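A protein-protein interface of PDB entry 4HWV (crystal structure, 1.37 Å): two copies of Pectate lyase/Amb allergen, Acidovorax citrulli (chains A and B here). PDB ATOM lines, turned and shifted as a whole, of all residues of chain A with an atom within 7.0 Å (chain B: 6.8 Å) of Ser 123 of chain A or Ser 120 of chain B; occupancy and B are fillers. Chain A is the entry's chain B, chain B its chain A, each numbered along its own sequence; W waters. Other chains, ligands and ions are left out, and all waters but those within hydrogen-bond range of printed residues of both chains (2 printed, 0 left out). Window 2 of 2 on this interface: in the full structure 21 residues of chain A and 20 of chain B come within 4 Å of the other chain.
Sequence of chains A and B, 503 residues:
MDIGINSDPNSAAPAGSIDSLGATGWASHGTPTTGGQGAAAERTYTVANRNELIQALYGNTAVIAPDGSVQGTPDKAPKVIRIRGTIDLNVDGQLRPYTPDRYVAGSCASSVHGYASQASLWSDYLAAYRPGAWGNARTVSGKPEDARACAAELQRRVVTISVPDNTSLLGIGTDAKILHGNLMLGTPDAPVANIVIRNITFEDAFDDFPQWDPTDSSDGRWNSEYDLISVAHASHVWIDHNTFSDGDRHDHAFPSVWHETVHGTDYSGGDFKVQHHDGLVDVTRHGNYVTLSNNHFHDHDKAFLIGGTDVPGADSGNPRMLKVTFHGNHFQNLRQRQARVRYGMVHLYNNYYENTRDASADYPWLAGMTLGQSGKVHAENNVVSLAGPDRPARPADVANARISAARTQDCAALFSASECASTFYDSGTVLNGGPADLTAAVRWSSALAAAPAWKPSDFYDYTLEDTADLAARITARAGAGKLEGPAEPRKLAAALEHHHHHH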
ATOM      1  N   TYR A 115     -20.843  11.125 -12.025  1.00  0.00           N
ATOM      2  CA  TYR A 115     -20.295  12.214 -12.845  1.00  0.00           C
ATOM      3  C   TYR A 115     -20.126  11.821 -14.302  1.00  0.00           C
ATOM      4  O   TYR A 115     -19.639  10.722 -14.615  1.00  0.00           O
ATOM      5  CB  TYR A 115     -18.980  12.747 -12.244  1.00  0.00           C
ATOM      6  CG  TYR A 115     -19.301  13.610 -11.063  1.00  0.00           C
ATOM      7  CD1 TYR A 115     -19.717  14.926 -11.256  1.00  0.00           C
ATOM      8  CD2 TYR A 115     -19.283  13.103  -9.759  1.00  0.00           C
ATOM      9  CE1 TYR A 115     -20.074  15.729 -10.193  1.00  0.00           C
ATOM     10  CE2 TYR A 115     -19.633  13.913  -8.676  1.00  0.00           C
ATOM     11  CZ  TYR A 115     -20.027  15.221  -8.918  1.00  0.00           C
ATOM     12  OH  TYR A 115     -20.391  16.015  -7.871  1.00  0.00           O
ATOM     13  N   GLN A 118     -15.198  15.328 -16.209  1.00  0.00           N
ATOM     14  CA  GLN A 118     -14.375  16.009 -15.226  1.00  0.00           C
ATOM     15  C   GLN A 118     -14.784  17.480 -15.040  1.00  0.00           C
ATOM     16  O   GLN A 118     -14.712  18.003 -13.935  1.00  0.00           O
ATOM     17  CB  GLN A 118     -12.888  15.864 -15.546  1.00  0.00           C
ATOM     18  CG  GLN A 118     -11.991  16.465 -14.460  1.00  0.00           C
ATOM     19  CD  GLN A 118     -11.602  17.912 -14.722  1.00  0.00           C
ATOM     20  OE1 GLN A 118     -11.561  18.367 -15.874  1.00  0.00           O
ATOM     21  NE2 GLN A 118     -11.264  18.633 -13.656  1.00  0.00           N
ATOM     22  N   ALA A 119     -15.215  18.151 -16.106  1.00  0.00           N
ATOM     23  CA  ALA A 119     -15.612  19.553 -15.973  1.00  0.00           C
ATOM     24  C   ALA A 119     -16.788  19.695 -14.994  1.00  0.00           C
ATOM     25  O   ALA A 119     -16.829  20.613 -14.178  1.00  0.00           O
ATOM     26  CB  ALA A 119     -15.954  20.165 -17.341  1.00  0.00           C
ATOM     27  N   SER A 120     -17.712  18.747 -15.038  1.00  0.00           N
ATOM     28  CA  SER A 120     -18.860  18.731 -14.137  1.00  0.00           C
ATOM     29  C   SER A 120     -18.420  18.483 -12.696  1.00  0.00           C
ATOM     30  O   SER A 120     -18.856  19.154 -11.758  1.00  0.00           O
ATOM     31  CB  SER A 120     -19.836  17.638 -14.578  1.00  0.00           C
ATOM     32  OG  SER A 120     -20.844  17.454 -13.610  1.00  0.00           O
ATOM     33  N   LEU A 121     -17.548  17.494 -12.523  1.00  0.00           N
ATOM     34  CA  LEU A 121     -17.011  17.202 -11.202  1.00  0.00           C
ATOM     35  C   LEU A 121     -16.331  18.439 -10.616  1.00  0.00           C
ATOM     36  O   LEU A 121     -16.573  18.808  -9.470  1.00  0.00           O
ATOM     37  CB  LEU A 121     -16.036  16.023 -11.271  1.00  0.00           C
ATOM     38  CG  LEU A 121     -15.253  15.776  -9.988  1.00  0.00           C
ATOM     39  CD1 LEU A 121     -16.196  15.557  -8.774  1.00  0.00           C
ATOM     40  CD2 LEU A 121     -14.287  14.597 -10.174  1.00  0.00           C
ATOM     41  N   TRP A 122     -15.483  19.074 -11.418  1.00  0.00           N
ATOM     42  CA  TRP A 122     -14.701  20.226 -10.954  1.00  0.00           C
ATOM     43  C   TRP A 122     -15.623  21.375 -10.542  1.00  0.00           C
ATOM     44  O   TRP A 122     -15.427  21.977  -9.492  1.00  0.00           O
ATOM     45  CB  TRP A 122     -13.743  20.650 -12.061  1.00  0.00           C
ATOM     46  CG  TRP A 122     -12.772  21.737 -11.746  1.00  0.00           C
ATOM     47  CD1 TRP A 122     -12.634  22.913 -12.436  1.00  0.00           C
ATOM     48  CD2 TRP A 122     -11.747  21.737 -10.726  1.00  0.00           C
ATOM     49  NE1 TRP A 122     -11.602  23.654 -11.892  1.00  0.00           N
ATOM     50  CE2 TRP A 122     -11.043  22.958 -10.847  1.00  0.00           C
ATOM     51  CE3 TRP A 122     -11.375  20.833  -9.710  1.00  0.00           C
ATOM     52  CZ2 TRP A 122      -9.976  23.294 -10.007  1.00  0.00           C
ATOM     53  CZ3 TRP A 122     -10.320  21.175  -8.875  1.00  0.00           C
ATOM     54  CH2 TRP A 122      -9.637  22.403  -9.025  1.00  0.00           C
ATOM     55  N   SER A 123     -16.641  21.665 -11.353  1.00  0.00           N
ATOM     56  CA  SER A 123     -17.595  22.706 -10.996  1.00  0.00           C
ATOM     57  C   SER A 123     -18.293  22.402  -9.659  1.00  0.00           C
ATOM     58  O   SER A 123     -18.443  23.290  -8.812  1.00  0.00           O
ATOM     59  CB  SER A 123     -18.609  22.881 -12.126  1.00  0.00           C
ATOM     60  OG  SER A 123     -19.516  23.915 -11.821  1.00  0.00           O
ATOM     61  N   ASP A 124     -18.755  21.164  -9.484  1.00  0.00           N
ATOM     62  CA  ASP A 124     -19.428  20.798  -8.242  1.00  0.00           C
ATOM     63  C   ASP A 124     -18.465  20.864  -7.057  1.00  0.00           C
ATOM     64  O   ASP A 124     -18.850  21.247  -5.948  1.00  0.00           O
ATOM     65  CB  ASP A 124     -19.952  19.352  -8.322  1.00  0.00           C
ATOM     66  CG  ASP A 124     -21.267  19.224  -9.007  1.00  0.00           C
ATOM     67  OD1 ASP A 124     -21.759  20.222  -9.584  1.00  0.00           O
ATOM     68  OD2 ASP A 124     -21.814  18.095  -8.960  1.00  0.00           O
ATOM     69  N   TYR A 125     -17.214  20.455  -7.279  1.00  0.00           N
ATOM     70  CA  TYR A 125     -16.213  20.435  -6.209  1.00  0.00           C
ATOM     71  C   TYR A 125     -15.980  21.848  -5.688  1.00  0.00           C
ATOM     72  O   TYR A 125     -15.943  22.097  -4.478  1.00  0.00           O
ATOM     73  CB  TYR A 125     -14.915  19.827  -6.754  1.00  0.00           C
ATOM     74  CG  TYR A 125     -13.906  19.429  -5.703  1.00  0.00           C
ATOM     75  CD1 TYR A 125     -12.937  20.334  -5.267  1.00  0.00           C
ATOM     76  CD2 TYR A 125     -13.908  18.149  -5.142  1.00  0.00           C
ATOM     77  CE1 TYR A 125     -12.000  19.981  -4.307  1.00  0.00           C
ATOM     78  CE2 TYR A 125     -12.975  17.784  -4.192  1.00  0.00           C
ATOM     79  CZ  TYR A 125     -12.019  18.707  -3.769  1.00  0.00           C
ATOM     80  OH  TYR A 125     -11.092  18.358  -2.810  1.00  0.00           O
ATOM     81  N   LEU A 126     -15.832  22.787  -6.612  1.00  0.00           N
ATOM     82  CA  LEU A 126     -15.596  24.183  -6.234  1.00  0.00           C
ATOM     83  C   LEU A 126     -16.815  24.781  -5.510  1.00  0.00           C
ATOM     84  O   LEU A 126     -16.664  25.480  -4.501  1.00  0.00           O
ATOM     85  CB  LEU A 126     -15.236  24.988  -7.485  1.00  0.00           C
ATOM     86  CG  LEU A 126     -13.771  24.959  -7.920  1.00  0.00           C
ATOM     87  CD1 LEU A 126     -12.973  23.731  -7.520  1.00  0.00           C
ATOM     88  CD2 LEU A 126     -13.580  25.386  -9.387  1.00  0.00           C
ATOM     89  N   ALA A 127     -18.016  24.485  -5.999  1.00  0.00           N
ATOM     90  CA  ALA A 127     -19.220  24.994  -5.352  1.00  0.00           C
ATOM     91  C   ALA A 127     -19.358  24.441  -3.935  1.00  0.00           C
ATOM     92  O   ALA A 127     -19.834  25.133  -3.044  1.00  0.00           O
ATOM     93  CB  ALA A 127     -20.458  24.633  -6.171  1.00  0.00           C
ATOM     94  N   ALA A 128     -18.984  23.181  -3.734  1.00  0.00           N
ATOM     95  CA  ALA A 128     -19.123  22.556  -2.420  1.00  0.00           C
ATOM     96  C   ALA A 128     -18.086  23.055  -1.427  1.00  0.00           C
ATOM     97  O   ALA A 128     -18.389  23.231  -0.243  1.00  0.00           O
ATOM     98  CB  ALA A 128     -18.995  21.054  -2.556  1.00  0.00           C
ATOM     99  N   PRO A 144     -18.722  15.214  -4.125  1.00  0.00           N
ATOM    100  CA  PRO A 144     -17.657  15.601  -5.062  1.00  0.00           C
ATOM    101  C   PRO A 144     -16.266  15.179  -4.571  1.00  0.00           C
ATOM    102  O   PRO A 144     -15.416  14.807  -5.384  1.00  0.00           O
ATOM    103  CB  PRO A 144     -17.789  17.129  -5.150  1.00  0.00           C
ATOM    104  CG  PRO A 144     -19.134  17.440  -4.623  1.00  0.00           C
ATOM    105  CD  PRO A 144     -19.505  16.372  -3.649  1.00  0.00           C
ATOM    106  N   ASP B 101     -11.523  33.227 -12.769  1.00  0.00           N
ATOM    107  CA  ASP B 101     -12.625  33.394 -11.820  1.00  0.00           C
ATOM    108  C   ASP B 101     -12.913  34.833 -11.454  1.00  0.00           C
ATOM    109  O   ASP B 101     -14.061  35.198 -11.246  1.00  0.00           O
ATOM    110  CB  ASP B 101     -12.438  32.524 -10.583  1.00  0.00           C
ATOM    111  CG  ASP B 101     -12.869  31.114 -10.843  1.00  0.00           C
ATOM    112  OD1 ASP B 101     -14.084  30.880 -10.737  1.00  0.00           O
ATOM    113  OD2 ASP B 101     -12.016  30.270 -11.202  1.00  0.00           O
ATOM    114  N   GLY B 114     -25.304  34.848 -13.901  1.00  0.00           N
ATOM    115  CA  GLY B 114     -25.382  34.052 -12.693  1.00  0.00           C
ATOM    116  C   GLY B 114     -24.305  33.004 -12.497  1.00  0.00           C
ATOM    117  O   GLY B 114     -24.439  32.151 -11.630  1.00  0.00           O
ATOM    118  N   TYR B 115     -23.248  33.028 -13.303  1.00  0.00           N
ATOM    119  CA  TYR B 115     -22.170  32.047 -13.130  1.00  0.00           C
ATOM    120  C   TYR B 115     -21.366  32.292 -11.863  1.00  0.00           C
ATOM    121  O   TYR B 115     -20.852  33.393 -11.654  1.00  0.00           O
ATOM    122  CB  TYR B 115     -21.257  32.001 -14.364  1.00  0.00           C
ATOM    123  CG  TYR B 115     -21.951  31.219 -15.458  1.00  0.00           C
ATOM    124  CD1 TYR B 115     -21.967  29.825 -15.422  1.00  0.00           C
ATOM    125  CD2 TYR B 115     -22.629  31.867 -16.499  1.00  0.00           C
ATOM    126  CE1 TYR B 115     -22.618  29.096 -16.378  1.00  0.00           C
ATOM    127  CE2 TYR B 115     -23.300  31.139 -17.459  1.00  0.00           C
ATOM    128  CZ  TYR B 115     -23.292  29.756 -17.395  1.00  0.00           C
ATOM    129  OH  TYR B 115     -23.961  29.043 -18.352  1.00  0.00           O
ATOM    130  N   ALA B 116     -21.259  31.257 -11.028  1.00  0.00           N
ATOM    131  CA  ALA B 116     -20.600  31.359  -9.732  1.00  0.00           C
ATOM    132  C   ALA B 116     -19.124  30.990  -9.806  1.00  0.00           C
ATOM    133  O   ALA B 116     -18.394  31.193  -8.841  1.00  0.00           O
ATOM    134  CB  ALA B 116     -21.294  30.476  -8.712  1.00  0.00           C
ATOM    135  N   SER B 117     -18.691  30.469 -10.953  1.00  0.00           N
ATOM    136  CA  SER B 117     -17.299  30.087 -11.148  1.00  0.00           C
ATOM    137  C   SER B 117     -16.988  29.973 -12.627  1.00  0.00           C
ATOM    138  O   SER B 117     -17.881  29.728 -13.453  1.00  0.00           O
ATOM    139  CB  SER B 117     -17.010  28.740 -10.481  1.00  0.00           C
ATOM    140  OG  SER B 117     -17.714  27.686 -11.132  1.00  0.00           O
ATOM    141  N   GLN B 118     -15.705  30.111 -12.951  1.00  0.00           N
ATOM    142  CA  GLN B 118     -15.212  29.769 -14.268  1.00  0.00           C
ATOM    143  C   GLN B 118     -15.478  28.283 -14.571  1.00  0.00           C
ATOM    144  O   GLN B 118     -15.860  27.929 -15.688  1.00  0.00           O
ATOM    145  CB  GLN B 118     -13.723  30.119 -14.374  1.00  0.00           C
ATOM    146  CG  GLN B 118     -12.940  29.424 -15.497  1.00  0.00           C
ATOM    147  CD  GLN B 118     -13.285  29.903 -16.889  1.00  0.00           C
ATOM    148  OE1 GLN B 118     -14.365  30.446 -17.139  1.00  0.00           O
ATOM    149  NE2 GLN B 118     -12.359  29.702 -17.813  1.00  0.00           N
ATOM    150  N   ALA B 119     -15.320  27.415 -13.575  1.00  0.00           N
ATOM    151  CA  ALA B 119     -15.534  25.990 -13.793  1.00  0.00           C
ATOM    152  C   ALA B 119     -16.959  25.731 -14.297  1.00  0.00           C
ATOM    153  O   ALA B 119     -17.181  24.923 -15.204  1.00  0.00           O
ATOM    154  CB  ALA B 119     -15.286  25.229 -12.506  1.00  0.00           C
ATOM    155  N   SER B 120     -17.927  26.399 -13.682  1.00  0.00           N
ATOM    156  CA  SER B 120     -19.318  26.228 -14.084  1.00  0.00           C
ATOM    157  C   SER B 120     -19.566  26.758 -15.501  1.00  0.00           C
ATOM    158  O   SER B 120     -20.228  26.106 -16.306  1.00  0.00           O
ATOM    159  CB  SER B 120     -20.237  26.913 -13.076  1.00  0.00           C
ATOM    160  OG  SER B 120     -21.570  26.930 -13.544  1.00  0.00           O
ATOM    161  N   LEU B 121     -19.026  27.935 -15.807  1.00  0.00           N
ATOM    162  CA  LEU B 121     -19.171  28.508 -17.135  1.00  0.00           C
ATOM    163  C   LEU B 121     -18.562  27.583 -18.180  1.00  0.00           C
ATOM    164  O   LEU B 121     -19.197  27.283 -19.198  1.00  0.00           O
ATOM    165  CB  LEU B 121     -18.520  29.892 -17.166  1.00  0.00           C
ATOM    166  CG  LEU B 121     -18.480  30.547 -18.563  1.00  0.00           C
ATOM    167  CD1 LEU B 121     -19.869  30.638 -19.210  1.00  0.00           C
ATOM    168  CD2 LEU B 121     -17.857  31.915 -18.438  1.00  0.00           C
ATOM    169  N   TRP B 122     -17.328  27.151 -17.936  1.00  0.00           N
ATOM    170  CA  TRP B 122     -16.628  26.305 -18.892  1.00  0.00           C
ATOM    171  C   TRP B 122     -17.364  24.982 -19.098  1.00  0.00           C
ATOM    172  O   TRP B 122     -17.538  24.543 -20.236  1.00  0.00           O
ATOM    173  CB  TRP B 122     -15.204  26.072 -18.393  1.00  0.00           C
ATOM    174  CG  TRP B 122     -14.289  25.282 -19.298  1.00  0.00           C
ATOM    175  CD1 TRP B 122     -13.719  24.084 -19.012  1.00  0.00           C
ATOM    176  CD2 TRP B 122     -13.811  25.660 -20.598  1.00  0.00           C
ATOM    177  NE1 TRP B 122     -12.905  23.688 -20.050  1.00  0.00           N
ATOM    178  CE2 TRP B 122     -12.950  24.635 -21.037  1.00  0.00           C
ATOM    179  CE3 TRP B 122     -14.034  26.761 -21.432  1.00  0.00           C
ATOM    180  CZ2 TRP B 122     -12.299  24.676 -22.266  1.00  0.00           C
ATOM    181  CZ3 TRP B 122     -13.386  26.800 -22.662  1.00  0.00           C
ATOM    182  CH2 TRP B 122     -12.537  25.759 -23.070  1.00  0.00           C
ATOM    183  N   SER B 123     -17.817  24.352 -18.011  1.00  0.00           N
ATOM    184  CA  SER B 123     -18.586  23.123 -18.138  1.00  0.00           C
ATOM    185  C   SER B 123     -19.829  23.351 -19.004  1.00  0.00           C
ATOM    186  O   SER B 123     -20.103  22.559 -19.917  1.00  0.00           O
ATOM    187  CB  SER B 123     -18.974  22.609 -16.758  1.00  0.00           C
ATOM    188  OG  SER B 123     -19.688  21.387 -16.860  1.00  0.00           O
ATOM    189  N   ASP B 124     -20.587  24.414 -18.711  1.00  0.00           N
ATOM    190  CA  ASP B 124     -21.789  24.731 -19.509  1.00  0.00           C
ATOM    191  C   ASP B 124     -21.450  25.038 -20.964  1.00  0.00           C
ATOM    192  O   ASP B 124     -22.196  24.680 -21.870  1.00  0.00           O
ATOM    193  CB  ASP B 124     -22.538  25.937 -18.938  1.00  0.00           C
ATOM    194  CG  ASP B 124     -23.452  25.582 -17.785  1.00  0.00           C
ATOM    195  OD1 ASP B 124     -23.386  24.446 -17.247  1.00  0.00           O
ATOM    196  OD2 ASP B 124     -24.237  26.477 -17.405  1.00  0.00           O
ATOM    197  N   TYR B 125     -20.337  25.726 -21.179  1.00  0.00           N
ATOM    198  CA  TYR B 125     -19.925  26.121 -22.518  1.00  0.00           C
ATOM    199  C   TYR B 125     -19.616  24.891 -23.374  1.00  0.00           C
ATOM    200  O   TYR B 125     -20.096  24.763 -24.509  1.00  0.00           O
ATOM    201  CB  TYR B 125     -18.709  27.071 -22.412  1.00  0.00           C
ATOM    202  CG  TYR B 125     -18.420  27.841 -23.674  1.00  0.00           C
ATOM    203  CD1 TYR B 125     -17.577  27.310 -24.645  1.00  0.00           C
ATOM    204  CD2 TYR B 125     -18.979  29.101 -23.895  1.00  0.00           C
ATOM    205  CE1 TYR B 125     -17.300  28.009 -25.820  1.00  0.00           C
ATOM    206  CE2 TYR B 125     -18.721  29.795 -25.056  1.00  0.00           C
ATOM    207  CZ  TYR B 125     -17.877  29.251 -26.015  1.00  0.00           C
ATOM    208  OH  TYR B 125     -17.602  29.922 -27.186  1.00  0.00           O
HETATM  209  O   HOH W   1     -15.387  22.845 -14.964  1.00  0.00           O
HETATM  210  O   HOH W   2     -18.802  26.076  -9.248  1.00  0.00           O
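Water W2 bridges OG of Ser 117 of chain B (2.7 Å) and O of Ser 123 of chain A (2.8 Å). Water W1 bridges O of Ala 119 of chain B (2.8 Å) and O of Ala 119 of chain A (2.8 Å).
Of the 13 printed residues of chain B, 3 touch a printed residue of chain A. Printed residues of chain B that touch a printed residue of chain A: Ala 119, Ser 120 and Ser 123. Hydrophobic or aromatic side chains of chain B within 4 Å of the printed part of chain A: Ala 119. Among the printed residues, 6 pairs touch across the chains. Among the printed residues, no Asp or Glu carboxylate lies within 4 Å of a Lys or Arg side-chain nitrogen of the other chain.
Ala 119 of chain A touches Ser 123 of chain B, and with the chains exchanged Ser 123 of chain A touches Ala 119 of chain B. Ser 120 of chain A touches Ser 123 of chain B, and with the chains exchanged Ser 123 of chain A touches Ser 120 of chain B. Trp 122 of chain A touches Ala 119 of chain B, but with the chains exchanged Ala 119 of chain A does not touch Trp 122 of chain B (4.8 Å). Positions printed for both chains: 115, 118, 119, 120, 121, 122, 123, 124 and 125. Of the 6 pairs that touch across the chains among the printed residues, 4 have their exchanged pair printed and touching as well.
The backbone NH of Ser 120 of chain B sits close to the side-chain hydroxyl of Ser 123 of chain A (3.5 Å).
OG of Ser 117 of chain B sits at hydrogen-bond distance from N of Ser 120 of chain B (2.9 Å). OG of Ser 117 of chain B lies close to N of Ala 119 of chain B, at 3.4 Å.
Ser 123 of chain B touches Ala 119 of chain A (OG to C, 3.8 Å). Ser 120 of chain A touches Ser 123 of chain B. Trp 122 of chain A touches Ala 119 of chain B. Ser 123 of chain A touches Ala 119 of chain B (CA to CB, 3.7 Å). Ala 119 of chain B touches Leu 126 of chain A.
Printed residues of chain B within 4 Å of Ser 123 of chain A: Ala 119 (3.7 Å) and Ser 120 (3.2 Å). Ser 120 of chain B touches just one residue of chain A: Ser 123 (3.2 Å). Printed residues of chain B within 4 Å of Ser 120 of chain A: Ser 123 (3.8 Å). Printed residues of chain A within 4 Å of Ser 123 of chain B: Ala 119 and Ser 120.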
